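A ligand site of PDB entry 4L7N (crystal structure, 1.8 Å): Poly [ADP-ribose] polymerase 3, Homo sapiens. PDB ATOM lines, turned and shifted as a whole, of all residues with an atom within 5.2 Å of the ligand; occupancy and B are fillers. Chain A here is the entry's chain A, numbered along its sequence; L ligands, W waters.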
ATOM      1  N   ASP A 109      -3.838  37.872 -15.759  1.00  0.00           N
ATOM      2  CA  ASP A 109      -4.702  36.748 -15.389  1.00  0.00           C
ATOM      3  C   ASP A 109      -5.685  36.389 -16.502  1.00  0.00           C
ATOM      4  O   ASP A 109      -5.940  35.192 -16.730  1.00  0.00           O
ATOM      5  CB  ASP A 109      -5.422  37.016 -14.061  1.00  0.00           C
ATOM      6  CG  ASP A 109      -4.464  37.011 -12.887  1.00  0.00           C
ATOM      7  OD1 ASP A 109      -3.336  36.543 -13.068  1.00  0.00           O
ATOM      8  OD2 ASP A 109      -4.855  37.509 -11.789  1.00  0.00           O
ATOM      9  N   LEU A 112      -3.829  34.461 -19.096  1.00  0.00           N
ATOM     10  CA  LEU A 112      -3.563  33.083 -18.595  1.00  0.00           C
ATOM     11  C   LEU A 112      -4.793  32.176 -18.810  1.00  0.00           C
ATOM     12  O   LEU A 112      -4.670  30.986 -19.232  1.00  0.00           O
ATOM     13  CB  LEU A 112      -3.151  33.088 -17.126  1.00  0.00           C
ATOM     14  CG  LEU A 112      -1.762  33.677 -16.834  1.00  0.00           C
ATOM     15  CD1 LEU A 112      -1.548  33.869 -15.338  1.00  0.00           C
ATOM     16  CD2 LEU A 112      -0.697  32.821 -17.400  1.00  0.00           C
ATOM     17  N   VAL A 113      -5.967  32.746 -18.577  1.00  0.00           N
ATOM     18  CA  VAL A 113      -7.233  32.032 -18.789  1.00  0.00           C
ATOM     19  C   VAL A 113      -7.424  31.835 -20.313  1.00  0.00           C
ATOM     20  O   VAL A 113      -7.694  30.725 -20.789  1.00  0.00           O
ATOM     21  CB  VAL A 113      -8.459  32.786 -18.177  1.00  0.00           C
ATOM     22  CG1 VAL A 113      -9.828  32.154 -18.684  1.00  0.00           C
ATOM     23  CG2 VAL A 113      -8.445  32.806 -16.685  1.00  0.00           C
ATOM     24  N   ALA A 115      -5.163  31.657 -22.637  1.00  0.00           N
ATOM     25  CA  ALA A 115      -4.167  30.641 -23.022  1.00  0.00           C
ATOM     26  C   ALA A 115      -4.688  29.237 -22.816  1.00  0.00           C
ATOM     27  O   ALA A 115      -4.439  28.361 -23.635  1.00  0.00           O
ATOM     28  CB  ALA A 115      -2.775  30.889 -22.234  1.00  0.00           C
ATOM     29  N   ASP A 116      -5.459  29.005 -21.767  1.00  0.00           N
ATOM     30  CA  ASP A 116      -6.071  27.700 -21.526  1.00  0.00           C
ATOM     31  C   ASP A 116      -7.298  27.450 -22.359  1.00  0.00           C
ATOM     32  O   ASP A 116      -7.603  26.297 -22.689  1.00  0.00           O
ATOM     33  CB  ASP A 116      -6.426  27.507 -20.051  1.00  0.00           C
ATOM     34  CG  ASP A 116      -5.204  27.079 -19.225  1.00  0.00           C
ATOM     35  OD1 ASP A 116      -4.137  26.732 -19.860  1.00  0.00           O
ATOM     36  OD2 ASP A 116      -5.325  27.052 -17.984  1.00  0.00           O
ATOM     37  N   TRP A 208      -8.180  22.437  -1.365  1.00  0.00           N
ATOM     38  CA  TRP A 208      -9.070  22.983  -2.427  1.00  0.00           C
ATOM     39  C   TRP A 208      -8.363  23.875  -3.440  1.00  0.00           C
ATOM     40  O   TRP A 208      -7.468  24.670  -3.106  1.00  0.00           O
ATOM     41  CB  TRP A 208     -10.213  23.763  -1.787  1.00  0.00           C
ATOM     42  CG  TRP A 208     -11.091  23.003  -0.882  1.00  0.00           C
ATOM     43  CD1 TRP A 208     -11.061  22.999   0.489  1.00  0.00           C
ATOM     44  CD2 TRP A 208     -12.093  22.073  -1.274  1.00  0.00           C
ATOM     45  NE1 TRP A 208     -12.041  22.171   0.961  1.00  0.00           N
ATOM     46  CE2 TRP A 208     -12.653  21.535  -0.099  1.00  0.00           C
ATOM     47  CE3 TRP A 208     -12.549  21.606  -2.514  1.00  0.00           C
ATOM     48  CZ2 TRP A 208     -13.681  20.601  -0.118  1.00  0.00           C
ATOM     49  CZ3 TRP A 208     -13.587  20.682  -2.554  1.00  0.00           C
ATOM     50  CH2 TRP A 208     -14.122  20.141  -1.353  1.00  0.00           C
ATOM     51  N   HIS A 209      -8.742  23.711  -4.719  1.00  0.00           N
ATOM     52  CA  HIS A 209      -8.397  24.627  -5.766  1.00  0.00           C
ATOM     53  C   HIS A 209      -9.621  24.899  -6.653  1.00  0.00           C
ATOM     54  O   HIS A 209     -10.034  24.053  -7.453  1.00  0.00           O
ATOM     55  CB  HIS A 209      -7.222  24.141  -6.584  1.00  0.00           C
ATOM     56  CG  HIS A 209      -6.724  25.137  -7.584  1.00  0.00           C
ATOM     57  ND1 HIS A 209      -5.755  26.080  -7.268  1.00  0.00           N
ATOM     58  CD2 HIS A 209      -7.076  25.356  -8.874  1.00  0.00           C
ATOM     59  CE1 HIS A 209      -5.516  26.823  -8.352  1.00  0.00           C
ATOM     60  NE2 HIS A 209      -6.309  26.410  -9.338  1.00  0.00           N
ATOM     61  N   GLY A 210     -10.201  26.082  -6.525  1.00  0.00           N
ATOM     62  CA  GLY A 210     -11.315  26.497  -7.347  1.00  0.00           C
ATOM     63  C   GLY A 210     -10.881  27.276  -8.560  1.00  0.00           C
ATOM     64  O   GLY A 210      -9.971  28.056  -8.524  1.00  0.00           O
ATOM     65  N   THR A 211     -11.616  27.081  -9.642  1.00  0.00           N
ATOM     66  CA  THR A 211     -11.263  27.725 -10.835  1.00  0.00           C
ATOM     67  C   THR A 211     -12.425  28.005 -11.784  1.00  0.00           C
ATOM     68  O   THR A 211     -13.467  27.624 -11.533  1.00  0.00           O
ATOM     69  CB  THR A 211     -10.262  26.844 -11.575  1.00  0.00           C
ATOM     70  OG1 THR A 211      -9.462  27.687 -12.362  1.00  0.00           O
ATOM     71  CG2 THR A 211     -10.987  25.924 -12.467  1.00  0.00           C
ATOM     72  N   ASN A 212     -12.084  28.703 -12.845  1.00  0.00           N
ATOM     73  CA  ASN A 212     -12.959  28.999 -13.978  1.00  0.00           C
ATOM     74  C   ASN A 212     -13.312  27.669 -14.689  1.00  0.00           C
ATOM     75  O   ASN A 212     -12.471  26.931 -14.946  1.00  0.00           O
ATOM     76  CB  ASN A 212     -12.144  29.776 -15.054  1.00  0.00           C
ATOM     77  CG  ASN A 212     -12.353  31.261 -15.053  1.00  0.00           C
ATOM     78  OD1 ASN A 212     -13.255  31.759 -15.646  1.00  0.00           O
ATOM     79  ND2 ASN A 212     -11.427  31.953 -14.501  1.00  0.00           N
ATOM     80  N   VAL A 215     -10.935  26.694 -17.658  1.00  0.00           N
ATOM     81  CA  VAL A 215      -9.574  26.161 -17.542  1.00  0.00           C
ATOM     82  C   VAL A 215      -9.563  24.715 -17.052  1.00  0.00           C
ATOM     83  O   VAL A 215      -8.497  24.129 -16.925  1.00  0.00           O
ATOM     84  CB  VAL A 215      -8.697  27.085 -16.685  1.00  0.00           C
ATOM     85  CG1 VAL A 215      -8.803  28.553 -17.192  1.00  0.00           C
ATOM     86  CG2 VAL A 215      -9.093  27.018 -15.267  1.00  0.00           C
ATOM     87  N   ARG A 225      -0.459  24.476 -12.945  1.00  0.00           N
ATOM     88  CA  ARG A 225       0.776  25.014 -13.498  1.00  0.00           C
ATOM     89  C   ARG A 225       1.091  26.393 -12.938  1.00  0.00           C
ATOM     90  O   ARG A 225       0.190  27.160 -12.487  1.00  0.00           O
ATOM     91  CB  ARG A 225       0.656  25.161 -15.017  1.00  0.00           C
ATOM     92  CG  ARG A 225       0.811  23.850 -15.791  1.00  0.00           C
ATOM     93  CD  ARG A 225      -0.076  23.846 -17.096  1.00  0.00           C
ATOM     94  NE  ARG A 225      -1.494  23.951 -16.718  1.00  0.00           N
ATOM     95  CZ  ARG A 225      -2.448  24.571 -17.433  1.00  0.00           C
ATOM     96  NH1 ARG A 225      -2.188  25.131 -18.611  1.00  0.00           N
ATOM     97  NH2 ARG A 225      -3.672  24.647 -16.954  1.00  0.00           N
ATOM     98  N   MET A 227       2.880  29.647 -14.418  1.00  0.00           N
ATOM     99  CA  MET A 227       3.336  30.272 -15.684  1.00  0.00           C
ATOM    100  C   MET A 227       4.076  31.558 -15.400  1.00  0.00           C
ATOM    101  O   MET A 227       3.877  32.154 -14.335  1.00  0.00           O
ATOM    102  CB  MET A 227       2.136  30.558 -16.602  1.00  0.00           C
ATOM    103  CG  MET A 227       1.377  29.340 -17.019  1.00  0.00           C
ATOM    104  SD  MET A 227       2.321  28.129 -17.990  1.00  0.00           S
ATOM    105  CE  MET A 227       3.091  29.186 -19.187  1.00  0.00           C
ATOM    106  N   SER A 230       2.150  34.438 -13.847  1.00  0.00           N
ATOM    107  CA  SER A 230       1.214  34.241 -12.729  1.00  0.00           C
ATOM    108  C   SER A 230       1.690  34.956 -11.465  1.00  0.00           C
ATOM    109  O   SER A 230       2.892  35.150 -11.260  1.00  0.00           O
ATOM    110  CB  SER A 230       0.888  32.803 -12.459  1.00  0.00           C
ATOM    111  OG  SER A 230       1.996  32.011 -12.339  1.00  0.00           O
ATOM    112  N   TYR A 239      -1.764  28.155  -5.825  1.00  0.00           N
ATOM    113  CA  TYR A 239      -2.549  28.546  -4.700  1.00  0.00           C
ATOM    114  C   TYR A 239      -3.629  27.526  -4.359  1.00  0.00           C
ATOM    115  O   TYR A 239      -4.381  27.060  -5.261  1.00  0.00           O
ATOM    116  CB  TYR A 239      -3.264  29.861  -4.995  1.00  0.00           C
ATOM    117  CG  TYR A 239      -2.344  31.061  -5.042  1.00  0.00           C
ATOM    118  CD1 TYR A 239      -2.362  31.973  -3.995  1.00  0.00           C
ATOM    119  CD2 TYR A 239      -1.507  31.334  -6.171  1.00  0.00           C
ATOM    120  CE1 TYR A 239      -1.549  33.062  -4.012  1.00  0.00           C
ATOM    121  CE2 TYR A 239      -0.657  32.475  -6.189  1.00  0.00           C
ATOM    122  CZ  TYR A 239      -0.691  33.334  -5.103  1.00  0.00           C
ATOM    123  OH  TYR A 239       0.130  34.455  -4.984  1.00  0.00           O
ATOM    124  N   PHE A 240      -3.718  27.191  -3.067  1.00  0.00           N
ATOM    125  CA  PHE A 240      -4.749  26.381  -2.518  1.00  0.00           C
ATOM    126  C   PHE A 240      -5.342  26.962  -1.235  1.00  0.00           C
ATOM    127  O   PHE A 240      -4.761  27.824  -0.595  1.00  0.00           O
ATOM    128  CB  PHE A 240      -4.203  24.992  -2.146  1.00  0.00           C
ATOM    129  CG  PHE A 240      -3.518  24.258  -3.272  1.00  0.00           C
ATOM    130  CD1 PHE A 240      -4.213  23.261  -4.011  1.00  0.00           C
ATOM    131  CD2 PHE A 240      -2.185  24.529  -3.602  1.00  0.00           C
ATOM    132  CE1 PHE A 240      -3.552  22.622  -5.084  1.00  0.00           C
ATOM    133  CE2 PHE A 240      -1.541  23.844  -4.599  1.00  0.00           C
ATOM    134  CZ  PHE A 240      -2.245  22.897  -5.356  1.00  0.00           C
ATOM    135  N   ALA A 241      -6.460  26.422  -0.843  1.00  0.00           N
ATOM    136  CA  ALA A 241      -7.111  26.789   0.405  1.00  0.00           C
ATOM    137  C   ALA A 241      -7.540  25.555   1.185  1.00  0.00           C
ATOM    138  O   ALA A 241      -7.923  24.530   0.607  1.00  0.00           O
ATOM    139  CB  ALA A 241      -8.295  27.661   0.152  1.00  0.00           C
ATOM    140  N   LYS A 246     -13.075  29.812   0.718  1.00  0.00           N
ATOM    141  CA  LYS A 246     -12.083  30.625   0.062  1.00  0.00           C
ATOM    142  C   LYS A 246     -11.907  30.238  -1.409  1.00  0.00           C
ATOM    143  O   LYS A 246     -11.971  31.087  -2.310  1.00  0.00           O
ATOM    144  CB  LYS A 246     -10.767  30.507   0.823  1.00  0.00           C
ATOM    145  CG  LYS A 246      -9.601  31.205   0.159  1.00  0.00           C
ATOM    146  CD  LYS A 246      -9.798  32.710   0.139  1.00  0.00           C
ATOM    147  CE  LYS A 246      -8.629  33.434  -0.551  1.00  0.00           C
ATOM    148  NZ  LYS A 246      -8.948  34.892  -0.824  1.00  0.00           N
ATOM    149  N   SER A 247     -11.754  28.943  -1.667  1.00  0.00           N
ATOM    150  CA  SER A 247     -11.567  28.481  -3.053  1.00  0.00           C
ATOM    151  C   SER A 247     -12.819  28.716  -3.884  1.00  0.00           C
ATOM    152  O   SER A 247     -12.744  28.973  -5.071  1.00  0.00           O
ATOM    153  CB  SER A 247     -11.259  26.999  -3.063  1.00  0.00           C
ATOM    154  OG  SER A 247      -9.881  26.857  -2.710  1.00  0.00           O
ATOM    155  N   TYR A 250     -13.243  31.718  -6.264  1.00  0.00           N
ATOM    156  CA  TYR A 250     -12.623  31.717  -7.564  1.00  0.00           C
ATOM    157  C   TYR A 250     -13.374  30.889  -8.594  1.00  0.00           C
ATOM    158  O   TYR A 250     -12.936  30.783  -9.756  1.00  0.00           O
ATOM    159  CB  TYR A 250     -11.150  31.288  -7.445  1.00  0.00           C
ATOM    160  CG  TYR A 250     -10.402  32.120  -6.432  1.00  0.00           C
ATOM    161  CD1 TYR A 250      -9.724  33.310  -6.813  1.00  0.00           C
ATOM    162  CD2 TYR A 250     -10.433  31.802  -5.097  1.00  0.00           C
ATOM    163  CE1 TYR A 250      -9.069  34.079  -5.917  1.00  0.00           C
ATOM    164  CE2 TYR A 250      -9.761  32.597  -4.145  1.00  0.00           C
ATOM    165  CZ  TYR A 250      -9.079  33.738  -4.579  1.00  0.00           C
ATOM    166  OH  TYR A 250      -8.431  34.508  -3.640  1.00  0.00           O
ATOM    167  N   SER A 338      -6.565  31.097   5.138  1.00  0.00           N
ATOM    168  CA  SER A 338      -5.219  30.680   4.695  1.00  0.00           C
ATOM    169  C   SER A 338      -5.092  30.465   3.195  1.00  0.00           C
ATOM    170  O   SER A 338      -6.017  29.965   2.515  1.00  0.00           O
ATOM    171  CB  SER A 338      -4.806  29.386   5.422  1.00  0.00           C
ATOM    172  OG  SER A 338      -4.755  29.603   6.829  1.00  0.00           O
ATOM    173  N   GLU A 339      -3.946  30.832   2.657  1.00  0.00           N
ATOM    174  CA  GLU A 339      -3.569  30.472   1.274  1.00  0.00           C
ATOM    175  C   GLU A 339      -2.325  29.610   1.364  1.00  0.00           C
ATOM    176  O   GLU A 339      -1.346  30.021   1.994  1.00  0.00           O
ATOM    177  CB  GLU A 339      -3.328  31.718   0.436  1.00  0.00           C
ATOM    178  CG  GLU A 339      -4.518  32.697   0.516  1.00  0.00           C
ATOM    179  CD  GLU A 339      -4.468  33.822  -0.491  1.00  0.00           C
ATOM    180  OE1 GLU A 339      -3.619  33.857  -1.366  1.00  0.00           O
ATOM    181  OE2 GLU A 339      -5.312  34.726  -0.337  1.00  0.00           O
HETATM  182  C1  LIG L   1      -4.123  31.204 -13.498  1.00  0.00           C
HETATM  183  C2  LIG L   1      -3.223  30.404 -14.211  1.00  0.00           C
HETATM  184  C3  LIG L   1      -3.707  29.568 -15.231  1.00  0.00           C
HETATM  185  S1  LIG L   1      -2.545  28.571 -16.228  1.00  0.00           S
HETATM  186  O1  LIG L   1      -1.260  29.404 -16.233  1.00  0.00           O
HETATM  187  O2  LIG L   1      -2.345  27.178 -15.643  1.00  0.00           O
HETATM  188  N1  LIG L   1      -3.162  28.496 -17.756  1.00  0.00           N
HETATM  189  C4  LIG L   1      -5.058  29.579 -15.561  1.00  0.00           C
HETATM  190  C5  LIG L   1      -5.953  30.355 -14.811  1.00  0.00           C
HETATM  191  C6  LIG L   1      -5.488  31.177 -13.774  1.00  0.00           C
HETATM  192  C7  LIG L   1      -6.386  32.007 -13.049  1.00  0.00           C
HETATM  193  C8  LIG L   1      -6.078  33.482 -13.308  1.00  0.00           C
HETATM  194  N2  LIG L   1      -6.218  31.902 -11.594  1.00  0.00           N
HETATM  195  C9  LIG L   1      -6.996  31.155 -10.875  1.00  0.00           C
HETATM  196  O3  LIG L   1      -7.881  30.445 -11.348  1.00  0.00           O
HETATM  197  C10 LIG L   1      -6.672  31.250  -9.392  1.00  0.00           C
HETATM  198  C11 LIG L   1      -7.675  30.368  -8.737  1.00  0.00           C
HETATM  199  C12 LIG L   1      -7.514  30.256  -7.331  1.00  0.00           C
HETATM  200  N3  LIG L   1      -6.826  31.118  -6.558  1.00  0.00           N
HETATM  201  C13 LIG L   1      -6.726  30.897  -5.189  1.00  0.00           C
HETATM  202  C14 LIG L   1      -6.051  31.850  -4.390  1.00  0.00           C
HETATM  203  C15 LIG L   1      -5.952  31.656  -3.032  1.00  0.00           C
HETATM  204  C16 LIG L   1      -6.549  30.561  -2.436  1.00  0.00           C
HETATM  205  C17 LIG L   1      -7.268  29.630  -3.247  1.00  0.00           C
HETATM  206  C18 LIG L   1      -7.333  29.811  -4.613  1.00  0.00           C
HETATM  207  C19 LIG L   1      -8.062  28.900  -5.400  1.00  0.00           C
HETATM  208  O4  LIG L   1      -8.700  27.947  -4.918  1.00  0.00           O
HETATM  209  N4  LIG L   1      -8.129  29.158  -6.756  1.00  0.00           N
HETATM  210  O   HOH W   1      -6.803  27.549 -11.890  1.00  0.00           O
HETATM  211  O   HOH W   2      -9.572  30.293 -13.065  1.00  0.00           O
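A nitrogen (N1) of the ligand lies within hydrogen-bond range of the side-chain carboxylate (OD2) of Asp 116 (2.6 Å). OG of Ser 247 is in hydrogen-bond range of O4 of the ligand (2.7 Å). N of Gly 210 is in hydrogen-bond range of O4 of the ligand (2.9 Å). The backbone carbonyl oxygen (O) of Gly 210 is in hydrogen-bond range of a nitrogen (N4) of the ligand, 2.8 Å away. O2 of the ligand lies within hydrogen-bond range of NH2 of Arg 225, 3.1 Å away. O of Leu 112 lies within hydrogen-bond range of N1 of the ligand, 3.3 Å away. The side-chain hydroxyl (OG1) of Thr 211 is in hydrogen-bond range of an oxygen (O3) of the ligand (3.3 Å).
Asp 109 touches the ligand (CB to C8, 3.7 Å). CG2 of Val 113 touches C5 of the ligand, 3.97 Å away. Trp 208 touches the ligand (O to O4, 3.9 Å). His 209 touches the ligand (CA to O4, 3.4 Å). CG of Met 227 touches O1 of the ligand, at 2.8 Å. Tyr 239 touches the ligand (CB to C14, 3.5 Å). Phe 240 touches the ligand (O to C16, 3.8 Å). Tyr 250 touches the ligand. Glu 339 touches the ligand. Of the 22 residues printed, 15 come within 4 Å of the ligand. The nearest printed residue that does not touch the ligand is Lys 246 (4.02 Å).
Water W2 lies within hydrogen-bond range of O3 of the ligand (2.4 Å), OG1 of Thr 211 (2.7 Å) and ND2 of Asn 212 (2.9 Å). Water W1 lies within hydrogen-bond range of OG1 of Thr 211 (2.7 Å), NE2 of His 209 (2.8 Å) and O3 of the ligand (3.1 Å).
NH1 of Arg 225 is in salt-bridge range of OD1 of Asp 116, 2.8 Å away. The backbone carbonyl oxygen (O) of Trp 208 lies close to the side-chain hydroxyl (OG) of Ser 247, 3.3 Å away. The side-chain hydroxyl (OG) of Ser 230 sits at hydrogen-bond distance from the backbone carbonyl oxygen (O) of Met 227, at 2.7 Å. ND1 of His 209 sits at hydrogen-bond distance from O of Tyr 239, at 2.6 Å. The side-chain hydroxyl (OH) of Tyr 250 sits at hydrogen-bond distance from the side-chain amino group (NZ) of Lys 246 (2.9 Å). The side-chain carboxylate (OE2) of Glu 339 lies within salt-bridge range of the side-chain amino group (NZ) of Lys 246, at 3.7 Å. N of Trp 208 is in hydrogen-bond range of O of Ala 241, at 2.9 Å.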
